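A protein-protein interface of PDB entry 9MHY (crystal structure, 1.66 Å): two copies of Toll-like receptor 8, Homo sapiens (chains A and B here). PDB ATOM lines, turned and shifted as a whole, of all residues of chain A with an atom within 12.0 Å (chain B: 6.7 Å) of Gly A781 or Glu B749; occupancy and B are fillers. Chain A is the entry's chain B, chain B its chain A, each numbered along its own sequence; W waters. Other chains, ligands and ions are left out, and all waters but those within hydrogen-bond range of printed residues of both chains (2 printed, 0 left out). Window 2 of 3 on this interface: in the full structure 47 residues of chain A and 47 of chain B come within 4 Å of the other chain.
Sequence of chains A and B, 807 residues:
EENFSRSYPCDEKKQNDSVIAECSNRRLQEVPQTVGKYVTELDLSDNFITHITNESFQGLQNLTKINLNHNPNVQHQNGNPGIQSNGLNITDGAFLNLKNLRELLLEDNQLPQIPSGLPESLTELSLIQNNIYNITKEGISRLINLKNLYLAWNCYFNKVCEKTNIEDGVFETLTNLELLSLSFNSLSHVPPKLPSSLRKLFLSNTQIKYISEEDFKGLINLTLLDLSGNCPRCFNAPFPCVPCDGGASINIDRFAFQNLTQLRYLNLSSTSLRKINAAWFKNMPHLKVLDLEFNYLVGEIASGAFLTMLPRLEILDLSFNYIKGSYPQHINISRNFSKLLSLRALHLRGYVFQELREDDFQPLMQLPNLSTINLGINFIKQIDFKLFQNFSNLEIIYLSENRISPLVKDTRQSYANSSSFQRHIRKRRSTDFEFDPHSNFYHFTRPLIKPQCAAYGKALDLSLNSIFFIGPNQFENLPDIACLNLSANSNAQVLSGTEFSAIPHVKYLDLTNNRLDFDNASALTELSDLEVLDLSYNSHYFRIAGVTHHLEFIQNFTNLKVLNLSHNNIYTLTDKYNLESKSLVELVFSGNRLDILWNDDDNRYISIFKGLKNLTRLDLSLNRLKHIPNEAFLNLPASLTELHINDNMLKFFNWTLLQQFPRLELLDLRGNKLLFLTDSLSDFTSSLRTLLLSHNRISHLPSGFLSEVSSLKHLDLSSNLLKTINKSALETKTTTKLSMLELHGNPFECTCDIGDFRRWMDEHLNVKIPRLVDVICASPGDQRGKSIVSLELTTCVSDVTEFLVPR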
ATOM      1  N   PRO A 747      12.681  12.771   1.255  1.00  0.00           N
ATOM      2  CA  PRO A 747      11.636  12.497   0.258  1.00  0.00           C
ATOM      3  C   PRO A 747      10.373  11.865   0.879  1.00  0.00           C
ATOM      4  O   PRO A 747      10.126  10.672   0.720  1.00  0.00           O
ATOM      5  CB  PRO A 747      12.358  11.552  -0.707  1.00  0.00           C
ATOM      6  CG  PRO A 747      13.247  10.752   0.185  1.00  0.00           C
ATOM      7  CD  PRO A 747      13.744  11.744   1.210  1.00  0.00           C
ATOM      8  N   PHE A 748       9.565  12.672   1.581  1.00  0.00           N
ATOM      9  CA  PHE A 748       8.384  12.164   2.284  1.00  0.00           C
ATOM     10  C   PHE A 748       7.276  11.678   1.383  1.00  0.00           C
ATOM     11  O   PHE A 748       7.001  12.274   0.339  1.00  0.00           O
ATOM     12  CB  PHE A 748       7.808  13.219   3.252  1.00  0.00           C
ATOM     13  CG  PHE A 748       8.604  13.383   4.523  1.00  0.00           C
ATOM     14  CD1 PHE A 748       8.529  12.440   5.533  1.00  0.00           C
ATOM     15  CD2 PHE A 748       9.472  14.446   4.682  1.00  0.00           C
ATOM     16  CE1 PHE A 748       9.290  12.572   6.688  1.00  0.00           C
ATOM     17  CE2 PHE A 748      10.202  14.594   5.855  1.00  0.00           C
ATOM     18  CZ  PHE A 748      10.126  13.644   6.836  1.00  0.00           C
ATOM     19  N   GLU A 749       6.623  10.590   1.814  1.00  0.00           N
ATOM     20  CA  GLU A 749       5.493   9.992   1.135  1.00  0.00           C
ATOM     21  C   GLU A 749       4.263  10.609   1.807  1.00  0.00           C
ATOM     22  O   GLU A 749       4.039  10.381   2.999  1.00  0.00           O
ATOM     23  CB  GLU A 749       5.505   8.463   1.313  1.00  0.00           C
ATOM     24  CG  GLU A 749       4.460   7.759   0.454  1.00  0.00           C
ATOM     25  CD  GLU A 749       4.689   6.278   0.203  1.00  0.00           C
ATOM     26  OE1 GLU A 749       3.733   5.609  -0.253  1.00  0.00           O
ATOM     27  OE2 GLU A 749       5.815   5.786   0.446  1.00  0.00           O
ATOM     28  N   CYS A 750       3.515  11.445   1.073  1.00  0.00           N
ATOM     29  CA  CYS A 750       2.357  12.145   1.612  1.00  0.00           C
ATOM     30  C   CYS A 750       1.047  11.479   1.267  1.00  0.00           C
ATOM     31  O   CYS A 750       0.270  11.958   0.446  1.00  0.00           O
ATOM     32  CB  CYS A 750       2.377  13.610   1.202  1.00  0.00           C
ATOM     33  SG  CYS A 750       3.773  14.531   1.900  1.00  0.00           S
ATOM     34  N   THR A 751       0.837  10.344   1.904  1.00  0.00           N
ATOM     35  CA  THR A 751      -0.392   9.558   1.868  1.00  0.00           C
ATOM     36  C   THR A 751      -0.923   9.595   3.337  1.00  0.00           C
ATOM     37  O   THR A 751      -0.325  10.269   4.187  1.00  0.00           O
ATOM     38  CB  THR A 751      -0.064   8.131   1.379  1.00  0.00           C
ATOM     39  OG1 THR A 751       0.850   7.536   2.306  1.00  0.00           O
ATOM     40  CG2 THR A 751       0.530   8.110  -0.025  1.00  0.00           C
ATOM     41  N   CYS A 752      -2.020   8.882   3.648  1.00  0.00           N
ATOM     42  CA  CYS A 752      -2.512   8.820   5.025  1.00  0.00           C
ATOM     43  C   CYS A 752      -1.468   8.187   5.991  1.00  0.00           C
ATOM     44  O   CYS A 752      -1.583   8.371   7.200  1.00  0.00           O
ATOM     45  CB  CYS A 752      -3.860   8.109   5.075  1.00  0.00           C
ATOM     46  SG  CYS A 752      -5.163   8.987   4.169  1.00  0.00           S
ATOM     47  N   ILE A 776       9.204  18.687   2.391  1.00  0.00           N
ATOM     48  CA  ILE A 776       8.369  18.503   1.202  1.00  0.00           C
ATOM     49  C   ILE A 776       8.008  17.056   0.852  1.00  0.00           C
ATOM     50  O   ILE A 776       8.764  16.128   1.121  1.00  0.00           O
ATOM     51  CB  ILE A 776       9.118  19.211   0.003  1.00  0.00           C
ATOM     52  CG1 ILE A 776       9.056  20.745   0.159  1.00  0.00           C
ATOM     53  CG2 ILE A 776       8.557  18.809  -1.368  1.00  0.00           C
ATOM     54  CD1 ILE A 776      10.165  21.525  -0.633  1.00  0.00           C
ATOM     55  N   CYS A 777       6.859  16.902   0.169  1.00  0.00           N
ATOM     56  CA  CYS A 777       6.375  15.630  -0.344  1.00  0.00           C
ATOM     57  C   CYS A 777       7.117  15.313  -1.646  1.00  0.00           C
ATOM     58  O   CYS A 777       7.094  16.123  -2.570  1.00  0.00           O
ATOM     59  CB  CYS A 777       4.872  15.693  -0.617  1.00  0.00           C
ATOM     60  SG  CYS A 777       3.856  16.216   0.784  1.00  0.00           S
ATOM     61  N   ALA A 778       7.678  14.115  -1.757  1.00  0.00           N
ATOM     62  CA  ALA A 778       8.266  13.623  -3.010  1.00  0.00           C
ATOM     63  C   ALA A 778       7.248  12.764  -3.789  1.00  0.00           C
ATOM     64  O   ALA A 778       7.414  12.586  -4.991  1.00  0.00           O
ATOM     65  CB  ALA A 778       9.504  12.800  -2.724  1.00  0.00           C
ATOM     66  N   SER A 779       6.214  12.214  -3.103  1.00  0.00           N
ATOM     67  CA  SER A 779       5.193  11.359  -3.701  1.00  0.00           C
ATOM     68  C   SER A 779       3.894  11.429  -2.882  1.00  0.00           C
ATOM     69  O   SER A 779       3.967  11.694  -1.684  1.00  0.00           O
ATOM     70  CB  SER A 779       5.689   9.914  -3.716  1.00  0.00           C
ATOM     71  OG  SER A 779       5.790   9.357  -2.416  1.00  0.00           O
ATOM     72  N   PRO A 780       2.708  11.108  -3.451  1.00  0.00           N
ATOM     73  CA  PRO A 780       2.432  10.835  -4.874  1.00  0.00           C
ATOM     74  C   PRO A 780       2.545  12.109  -5.729  1.00  0.00           C
ATOM     75  O   PRO A 780       2.805  13.197  -5.206  1.00  0.00           O
ATOM     76  CB  PRO A 780       1.018  10.243  -4.833  1.00  0.00           C
ATOM     77  CG  PRO A 780       0.367  10.926  -3.675  1.00  0.00           C
ATOM     78  CD  PRO A 780       1.461  11.155  -2.660  1.00  0.00           C
ATOM     79  N   GLY A 781       2.380  11.968  -7.041  1.00  0.00           N
ATOM     80  CA  GLY A 781       2.488  13.083  -7.981  1.00  0.00           C
ATOM     81  C   GLY A 781       1.671  14.311  -7.628  1.00  0.00           C
ATOM     82  O   GLY A 781       2.171  15.432  -7.702  1.00  0.00           O
ATOM     83  N   ASP A 782       0.413  14.108  -7.234  1.00  0.00           N
ATOM     84  CA  ASP A 782      -0.481  15.210  -6.849  1.00  0.00           C
ATOM     85  C   ASP A 782      -0.007  16.030  -5.628  1.00  0.00           C
ATOM     86  O   ASP A 782      -0.423  17.182  -5.487  1.00  0.00           O
ATOM     87  CB  ASP A 782      -1.907  14.692  -6.606  1.00  0.00           C
ATOM     88  CG  ASP A 782      -1.993  13.495  -5.677  1.00  0.00           C
ATOM     89  OD1 ASP A 782      -1.567  12.391  -6.091  1.00  0.00           O
ATOM     90  OD2 ASP A 782      -2.505  13.656  -4.544  1.00  0.00           O
ATOM     91  N   GLN A 783       0.846  15.446  -4.754  1.00  0.00           N
ATOM     92  CA  GLN A 783       1.362  16.126  -3.562  1.00  0.00           C
ATOM     93  C   GLN A 783       2.810  16.611  -3.701  1.00  0.00           C
ATOM     94  O   GLN A 783       3.261  17.371  -2.847  1.00  0.00           O
ATOM     95  CB  GLN A 783       1.244  15.212  -2.329  1.00  0.00           C
ATOM     96  CG  GLN A 783      -0.170  14.696  -2.064  1.00  0.00           C
ATOM     97  CD  GLN A 783      -1.166  15.817  -1.865  1.00  0.00           C
ATOM     98  OE1 GLN A 783      -0.849  16.869  -1.295  1.00  0.00           O
ATOM     99  NE2 GLN A 783      -2.394  15.622  -2.318  1.00  0.00           N
ATOM    100  N   ARG A 784       3.536  16.183  -4.751  1.00  0.00           N
ATOM    101  CA  ARG A 784       4.927  16.589  -4.984  1.00  0.00           C
ATOM    102  C   ARG A 784       5.108  18.119  -4.957  1.00  0.00           C
ATOM    103  O   ARG A 784       4.279  18.850  -5.500  1.00  0.00           O
ATOM    104  CB  ARG A 784       5.431  15.989  -6.311  1.00  0.00           C
ATOM    105  CG  ARG A 784       6.797  16.498  -6.797  1.00  0.00           C
ATOM    106  CD  ARG A 784       7.682  15.442  -7.455  1.00  0.00           C
ATOM    107  NE  ARG A 784       6.972  14.490  -8.320  1.00  0.00           N
ATOM    108  CZ  ARG A 784       7.537  13.430  -8.894  1.00  0.00           C
ATOM    109  NH1 ARG A 784       6.815  12.614  -9.652  1.00  0.00           N
ATOM    110  NH2 ARG A 784       8.823  13.173  -8.711  1.00  0.00           N
ATOM    111  N   GLY A 785       6.156  18.573  -4.271  1.00  0.00           N
ATOM    112  CA  GLY A 785       6.467  19.990  -4.120  1.00  0.00           C
ATOM    113  C   GLY A 785       5.820  20.667  -2.924  1.00  0.00           C
ATOM    114  O   GLY A 785       6.287  21.723  -2.490  1.00  0.00           O
ATOM    115  N   LYS A 786       4.743  20.093  -2.379  1.00  0.00           N
ATOM    116  CA  LYS A 786       4.033  20.692  -1.247  1.00  0.00           C
ATOM    117  C   LYS A 786       4.644  20.302   0.089  1.00  0.00           C
ATOM    118  O   LYS A 786       5.287  19.262   0.191  1.00  0.00           O
ATOM    119  CB  LYS A 786       2.563  20.250  -1.261  1.00  0.00           C
ATOM    120  CG  LYS A 786       1.808  20.629  -2.529  1.00  0.00           C
ATOM    121  CD  LYS A 786       0.350  20.191  -2.451  1.00  0.00           C
ATOM    122  CE  LYS A 786      -0.494  20.848  -3.515  1.00  0.00           C
ATOM    123  NZ  LYS A 786      -1.108  22.117  -3.025  1.00  0.00           N
ATOM    124  N   SER A 787       4.410  21.111   1.127  1.00  0.00           N
ATOM    125  CA  SER A 787       4.876  20.779   2.470  1.00  0.00           C
ATOM    126  C   SER A 787       4.015  19.634   3.031  1.00  0.00           C
ATOM    127  O   SER A 787       2.838  19.513   2.684  1.00  0.00           O
ATOM    128  CB  SER A 787       4.780  21.991   3.392  1.00  0.00           C
ATOM    129  OG  SER A 787       5.206  21.677   4.709  1.00  0.00           O
ATOM    130  N   SER A 790       0.464  20.266   4.441  1.00  0.00           N
ATOM    131  CA  SER A 790      -0.677  20.493   3.539  1.00  0.00           C
ATOM    132  C   SER A 790      -1.424  19.157   3.305  1.00  0.00           C
ATOM    133  O   SER A 790      -0.857  18.092   3.542  1.00  0.00           O
ATOM    134  CB  SER A 790      -0.193  21.064   2.211  1.00  0.00           C
ATOM    135  OG  SER A 790       0.512  22.275   2.433  1.00  0.00           O
ATOM    136  N   LEU A 791      -2.683  19.200   2.835  1.00  0.00           N
ATOM    137  CA  LEU A 791      -3.518  17.984   2.656  1.00  0.00           C
ATOM    138  C   LEU A 791      -3.891  17.442   4.055  1.00  0.00           C
ATOM    139  O   LEU A 791      -2.993  17.198   4.864  1.00  0.00           O
ATOM    140  CB  LEU A 791      -2.834  16.893   1.745  1.00  0.00           C
ATOM    141  CG  LEU A 791      -2.391  15.517   2.362  1.00  0.00           C
ATOM    142  CD1 LEU A 791      -3.546  14.552   2.438  1.00  0.00           C
ATOM    143  CD2 LEU A 791      -1.290  14.877   1.559  1.00  0.00           C
ATOM    144  N   LEU B 722      12.858  16.014 -14.114  1.00  0.00           N
ATOM    145  CA  LEU B 722      11.855  15.505 -15.034  1.00  0.00           C
ATOM    146  C   LEU B 722      11.002  14.447 -14.338  1.00  0.00           C
ATOM    147  O   LEU B 722      11.552  13.468 -13.837  1.00  0.00           O
ATOM    148  CB  LEU B 722      12.513  14.873 -16.272  1.00  0.00           C
ATOM    149  CG  LEU B 722      13.370  15.787 -17.146  1.00  0.00           C
ATOM    150  CD1 LEU B 722      14.116  14.969 -18.193  1.00  0.00           C
ATOM    151  CD2 LEU B 722      12.523  16.880 -17.803  1.00  0.00           C
ATOM    152  N   LYS B 723       9.670  14.654 -14.307  1.00  0.00           N
ATOM    153  CA  LYS B 723       8.705  13.713 -13.735  1.00  0.00           C
ATOM    154  C   LYS B 723       8.239  12.731 -14.837  1.00  0.00           C
ATOM    155  O   LYS B 723       7.877  11.603 -14.543  1.00  0.00           O
ATOM    156  CB  LYS B 723       7.493  14.467 -13.159  1.00  0.00           C
ATOM    157  CG  LYS B 723       7.830  15.430 -12.020  1.00  0.00           C
ATOM    158  CD  LYS B 723       6.664  16.363 -11.669  1.00  0.00           C
ATOM    159  CE  LYS B 723       5.414  15.622 -11.262  1.00  0.00           C
ATOM    160  NZ  LYS B 723       4.490  16.464 -10.445  1.00  0.00           N
ATOM    161  N   THR B 724       8.223  13.163 -16.108  1.00  0.00           N
ATOM    162  CA  THR B 724       7.833  12.324 -17.241  1.00  0.00           C
ATOM    163  C   THR B 724       8.335  12.962 -18.568  1.00  0.00           C
ATOM    164  O   THR B 724       8.914  14.047 -18.550  1.00  0.00           O
ATOM    165  CB  THR B 724       6.289  12.138 -17.248  1.00  0.00           C
ATOM    166  OG1 THR B 724       5.965  11.180 -18.258  1.00  0.00           O
ATOM    167  CG2 THR B 724       5.543  13.450 -17.508  1.00  0.00           C
ATOM    168  N   ASN B 746      16.597  11.401 -12.586  1.00  0.00           N
ATOM    169  CA  ASN B 746      15.392  12.237 -12.670  1.00  0.00           C
ATOM    170  C   ASN B 746      14.291  11.610 -11.814  1.00  0.00           C
ATOM    171  O   ASN B 746      14.152  10.387 -11.795  1.00  0.00           O
ATOM    172  CB  ASN B 746      14.913  12.388 -14.117  1.00  0.00           C
ATOM    173  CG  ASN B 746      15.724  13.391 -14.905  1.00  0.00           C
ATOM    174  OD1 ASN B 746      15.517  14.598 -14.773  1.00  0.00           O
ATOM    175  ND2 ASN B 746      16.677  12.921 -15.707  1.00  0.00           N
ATOM    176  N   PRO B 747      13.502  12.418 -11.083  1.00  0.00           N
ATOM    177  CA  PRO B 747      12.455  11.846 -10.224  1.00  0.00           C
ATOM    178  C   PRO B 747      11.201  11.455 -11.014  1.00  0.00           C
ATOM    179  O   PRO B 747      10.177  12.120 -10.945  1.00  0.00           O
ATOM    180  CB  PRO B 747      12.209  12.981  -9.230  1.00  0.00           C
ATOM    181  CG  PRO B 747      12.374  14.213 -10.056  1.00  0.00           C
ATOM    182  CD  PRO B 747      13.534  13.892 -10.974  1.00  0.00           C
ATOM    183  N   PHE B 748      11.311  10.406 -11.825  1.00  0.00           N
ATOM    184  CA  PHE B 748      10.212   9.955 -12.679  1.00  0.00           C
ATOM    185  C   PHE B 748       8.979   9.490 -11.887  1.00  0.00           C
ATOM    186  O   PHE B 748       9.121   8.868 -10.841  1.00  0.00           O
ATOM    187  CB  PHE B 748      10.689   8.815 -13.602  1.00  0.00           C
ATOM    188  CG  PHE B 748      11.527   9.281 -14.770  1.00  0.00           C
ATOM    189  CD1 PHE B 748      10.949   9.941 -15.836  1.00  0.00           C
ATOM    190  CD2 PHE B 748      12.887   9.041 -14.808  1.00  0.00           C
ATOM    191  CE1 PHE B 748      11.725  10.404 -16.891  1.00  0.00           C
ATOM    192  CE2 PHE B 748      13.653   9.477 -15.882  1.00  0.00           C
ATOM    193  CZ  PHE B 748      13.074  10.178 -16.902  1.00  0.00           C
ATOM    194  N   GLU B 749       7.778   9.818 -12.408  1.00  0.00           N
ATOM    195  CA  GLU B 749       6.478   9.442 -11.877  1.00  0.00           C
ATOM    196  C   GLU B 749       6.110   8.179 -12.646  1.00  0.00           C
ATOM    197  O   GLU B 749       5.943   8.231 -13.865  1.00  0.00           O
ATOM    198  CB  GLU B 749       5.448  10.553 -12.127  1.00  0.00           C
ATOM    199  CG  GLU B 749       4.117  10.303 -11.429  1.00  0.00           C
ATOM    200  CD  GLU B 749       3.224  11.514 -11.231  1.00  0.00           C
ATOM    201  OE1 GLU B 749       2.029  11.315 -10.915  1.00  0.00           O
ATOM    202  OE2 GLU B 749       3.712  12.658 -11.379  1.00  0.00           O
ATOM    203  N   CYS B 750       6.065   7.044 -11.952  1.00  0.00           N
ATOM    204  CA  CYS B 750       5.800   5.753 -12.562  1.00  0.00           C
ATOM    205  C   CYS B 750       4.374   5.307 -12.400  1.00  0.00           C
ATOM    206  O   CYS B 750       4.071   4.379 -11.659  1.00  0.00           O
ATOM    207  CB  CYS B 750       6.789   4.716 -12.049  1.00  0.00           C
ATOM    208  SG  CYS B 750       8.478   4.995 -12.632  1.00  0.00           S
ATOM    209  N   THR B 751       3.506   5.992 -13.126  1.00  0.00           N
ATOM    210  CA  THR B 751       2.085   5.707 -13.281  1.00  0.00           C
ATOM    211  C   THR B 751       1.920   5.366 -14.792  1.00  0.00           C
ATOM    212  O   THR B 751       2.923   5.324 -15.519  1.00  0.00           O
ATOM    213  CB  THR B 751       1.268   6.946 -12.843  1.00  0.00           C
ATOM    214  OG1 THR B 751       1.621   8.041 -13.693  1.00  0.00           O
ATOM    215  CG2 THR B 751       1.502   7.315 -11.383  1.00  0.00           C
ATOM    216  N   CYS B 752       0.689   5.135 -15.276  1.00  0.00           N
ATOM    217  CA  CYS B 752       0.475   4.885 -16.701  1.00  0.00           C
ATOM    218  C   CYS B 752       0.912   6.099 -17.578  1.00  0.00           C
ATOM    219  O   CYS B 752       1.130   5.927 -18.771  1.00  0.00           O
ATOM    220  CB  CYS B 752      -0.970   4.468 -16.954  1.00  0.00           C
ATOM    221  SG  CYS B 752      -1.418   2.909 -16.140  1.00  0.00           S
ATOM    222  N   ASP B 753       1.160   7.283 -16.968  1.00  0.00           N
ATOM    223  CA  ASP B 753       1.650   8.466 -17.679  1.00  0.00           C
ATOM    224  C   ASP B 753       3.073   8.265 -18.243  1.00  0.00           C
ATOM    225  O   ASP B 753       3.457   8.985 -19.160  1.00  0.00           O
ATOM    226  CB  ASP B 753       1.626   9.700 -16.760  1.00  0.00           C
ATOM    227  CG  ASP B 753       0.248  10.112 -16.276  1.00  0.00           C
ATOM    228  OD1 ASP B 753       0.151  10.639 -15.143  1.00  0.00           O
ATOM    229  OD2 ASP B 753      -0.736   9.902 -17.025  1.00  0.00           O
ATOM    230  N   ILE B 754       3.867   7.326 -17.698  1.00  0.00           N
ATOM    231  CA  ILE B 754       5.202   7.034 -18.255  1.00  0.00           C
ATOM    232  C   ILE B 754       5.119   6.048 -19.464  1.00  0.00           C
ATOM    233  O   ILE B 754       6.138   5.821 -20.110  1.00  0.00           O
ATOM    234  CB  ILE B 754       6.178   6.501 -17.154  1.00  0.00           C
ATOM    235  CG1 ILE B 754       7.665   6.711 -17.533  1.00  0.00           C
ATOM    236  CG2 ILE B 754       5.931   5.029 -16.874  1.00  0.00           C
ATOM    237  CD1 ILE B 754       8.151   8.118 -17.421  1.00  0.00           C
ATOM    238  N   ILE B 776      15.328   5.768 -12.248  1.00  0.00           N
ATOM    239  CA  ILE B 776      14.468   5.278 -11.159  1.00  0.00           C
ATOM    240  C   ILE B 776      13.161   6.056 -10.920  1.00  0.00           C
ATOM    241  O   ILE B 776      13.096   7.270 -11.104  1.00  0.00           O
ATOM    242  CB  ILE B 776      15.369   5.274  -9.858  1.00  0.00           C
ATOM    243  CG1 ILE B 776      16.442   4.167  -9.955  1.00  0.00           C
ATOM    244  CG2 ILE B 776      14.554   5.087  -8.576  1.00  0.00           C
ATOM    245  CD1 ILE B 776      17.739   4.432  -9.080  1.00  0.00           C
ATOM    246  N   CYS B 777      12.144   5.337 -10.414  1.00  0.00           N
ATOM    247  CA  CYS B 777      10.848   5.894 -10.047  1.00  0.00           C
ATOM    248  C   CYS B 777      10.986   6.580  -8.699  1.00  0.00           C
ATOM    249  O   CYS B 777      11.419   5.934  -7.747  1.00  0.00           O
ATOM    250  CB  CYS B 777       9.792   4.791  -9.951  1.00  0.00           C
ATOM    251  SG  CYS B 777       9.589   3.793 -11.446  1.00  0.00           S
ATOM    252  N   ALA B 778      10.545   7.833  -8.587  1.00  0.00           N
ATOM    253  CA  ALA B 778      10.486   8.538  -7.305  1.00  0.00           C
ATOM    254  C   ALA B 778       9.081   8.420  -6.677  1.00  0.00           C
ATOM    255  O   ALA B 778       8.949   8.604  -5.472  1.00  0.00           O
ATOM    256  CB  ALA B 778      10.831  10.003  -7.488  1.00  0.00           C
ATOM    257  N   SER B 779       8.035   8.141  -7.493  1.00  0.00           N
ATOM    258  CA  SER B 779       6.648   8.027  -7.051  1.00  0.00           C
ATOM    259  C   SER B 779       5.860   7.114  -8.006  1.00  0.00           C
ATOM    260  O   SER B 779       6.235   7.022  -9.172  1.00  0.00           O
ATOM    261  CB  SER B 779       6.003   9.413  -7.048  1.00  0.00           C
ATOM    262  OG  SER B 779       5.837   9.940  -8.353  1.00  0.00           O
ATOM    263  N   PRO B 780       4.726   6.503  -7.586  1.00  0.00           N
ATOM    264  CA  PRO B 780       4.181   6.448  -6.217  1.00  0.00           C
ATOM    265  C   PRO B 780       5.044   5.561  -5.301  1.00  0.00           C
ATOM    266  O   PRO B 780       6.035   4.977  -5.743  1.00  0.00           O
ATOM    267  CB  PRO B 780       2.763   5.903  -6.441  1.00  0.00           C
ATOM    268  CG  PRO B 780       2.895   5.011  -7.630  1.00  0.00           C
ATOM    269  CD  PRO B 780       3.955   5.641  -8.507  1.00  0.00           C
ATOM    270  N   ILE B 788      12.508   2.569 -14.262  1.00  0.00           N
ATOM    271  CA  ILE B 788      11.291   2.821 -15.034  1.00  0.00           C
ATOM    272  C   ILE B 788      11.005   1.662 -16.011  1.00  0.00           C
ATOM    273  O   ILE B 788       9.846   1.389 -16.294  1.00  0.00           O
ATOM    274  CB  ILE B 788      11.308   4.207 -15.745  1.00  0.00           C
ATOM    275  CG1 ILE B 788      12.312   4.250 -16.919  1.00  0.00           C
ATOM    276  CG2 ILE B 788      11.574   5.337 -14.729  1.00  0.00           C
ATOM    277  CD1 ILE B 788      12.209   5.503 -17.763  1.00  0.00           C
ATOM    278  N   LEU B 791       8.747  -1.286 -14.507  1.00  0.00           N
ATOM    279  CA  LEU B 791       7.331  -1.040 -14.225  1.00  0.00           C
ATOM    280  C   LEU B 791       6.414  -1.968 -15.051  1.00  0.00           C
ATOM    281  O   LEU B 791       6.714  -2.255 -16.212  1.00  0.00           O
ATOM    282  CB  LEU B 791       7.006   0.447 -14.485  1.00  0.00           C
ATOM    283  CG  LEU B 791       5.573   0.923 -14.245  1.00  0.00           C
ATOM    284  CD1 LEU B 791       5.165   0.774 -12.794  1.00  0.00           C
ATOM    285  CD2 LEU B 791       5.406   2.356 -14.695  1.00  0.00           C
HETATM  286  O   HOH W   1       7.402   7.237  -3.756  1.00  0.00           O
HETATM  287  O   HOH W   2       2.335   9.444  -8.560  1.00  0.00           O
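Water W1 lies within hydrogen-bond range of O of Ala B778, OG of Ser A779 and O of Pro B780. Water W2 lies within hydrogen-bond range of the backbone NH (N) of Gly A781 (2.9 Å) and the side-chain carboxylate (OE1) of Glu B749 (3.0 Å).
Hydrophobic or aromatic side chains of chain B that line the printed part of chain A: Pro B747 and Ala B778. Of the 20 printed residues of chain A, 3 touch a printed residue of chain B. Among the printed residues, 9 pairs touch across the chains. Among the printed residues, Asp or Glu carboxylates within 4 Å of a Lys or Arg side-chain nitrogen of the other chain: Arg A784 with Glu B749.
Ser A779 touches Ala B778, but with the chains exchanged Ala A778 does not touch Ser B779 (4.04 Å). Ser B779 touches its own counterpart, Ser A779. Of the 9 pairs that touch across the chains among the printed residues, 1 has its exchanged pair printed and touching as well.
The backbone carbonyl oxygen of Pro B747 lies within hydrogen-bond range of the guanidinium group of Arg A784. The side-chain carboxylate of Glu B749 lies within salt-bridge range of the guanidinium group of Arg A784 (3.6 Å). The side-chain hydroxyl (OG) of Ser B779 lies within hydrogen-bond range of the guanidinium group (NH1) of Arg A784, at 3.1 Å.
Among the printed residues, pairs that only touch across the chains: Ser A779 with Ser B779, Gly A781 with Glu B749, Arg A784 with Lys B723, Gly A781 with Lys B723, Ser A779 with Ala B778 and Arg A784 with Ala B778.
The side-chain amino group of Lys B723 is in salt-bridge range of the side-chain carboxylate of Glu B749, at 3.995 Å. The backbone NH (N) of Ala B778 lies within hydrogen-bond range of the backbone carbonyl oxygen (O) of Phe B748 (2.9 Å). The backbone NH of Cys B750 lies within hydrogen-bond range of the backbone carbonyl oxygen of Ser B779 (2.8 Å). The backbone NH (N) of Cys A750 lies within hydrogen-bond range of the backbone carbonyl oxygen (O) of Ser A779 (2.8 Å). SG of Cys B750 forms a disulfide with SG of Cys B777, 2.0 Å away. The side-chain sulfur (SG) of Cys A750 forms a disulfide with the side-chain sulfur (SG) of Cys A777 (2.0 Å).
Of the printed residues of chain B, Ser A779 touches Ala B778 (3.9 Å) and Ser B779 (3.4 Å). Gly A781 touches two residues of chain B. Of the printed residues of chain B, Arg A784 touches Lys B723, Pro B747, Glu B749, Ala B778 and Ser B779. Of chain A, only Gly A781 (3.7 Å) and Arg A784 (3.5 Å) come within 4 Å of Lys B723. No residue of chain A comes within 4 Å of Thr B724. Of chain A, only Arg A784 comes within 4 Å of Pro B747. No residue of chain A comes within 4 Å of Phe B748. No residue of chain A comes within 4 Å of Thr B751. No residue of chain A comes within 4 Å of Asp B753. No residue of chain A comes within 4 Å of Ile B754. Of the printed residues of chain A, Ala B778 touches Ser A779 and Arg A784. Ser B779 touches two residues of chain A. Ile B788 touches none of the printed residues of chain A. The nearest residue of chain B that does not touch Gly A781 is Ser B779 (4.2 Å). The nearest residue of chain A that does not touch Glu B749 is Asp A782 (4.9 Å).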
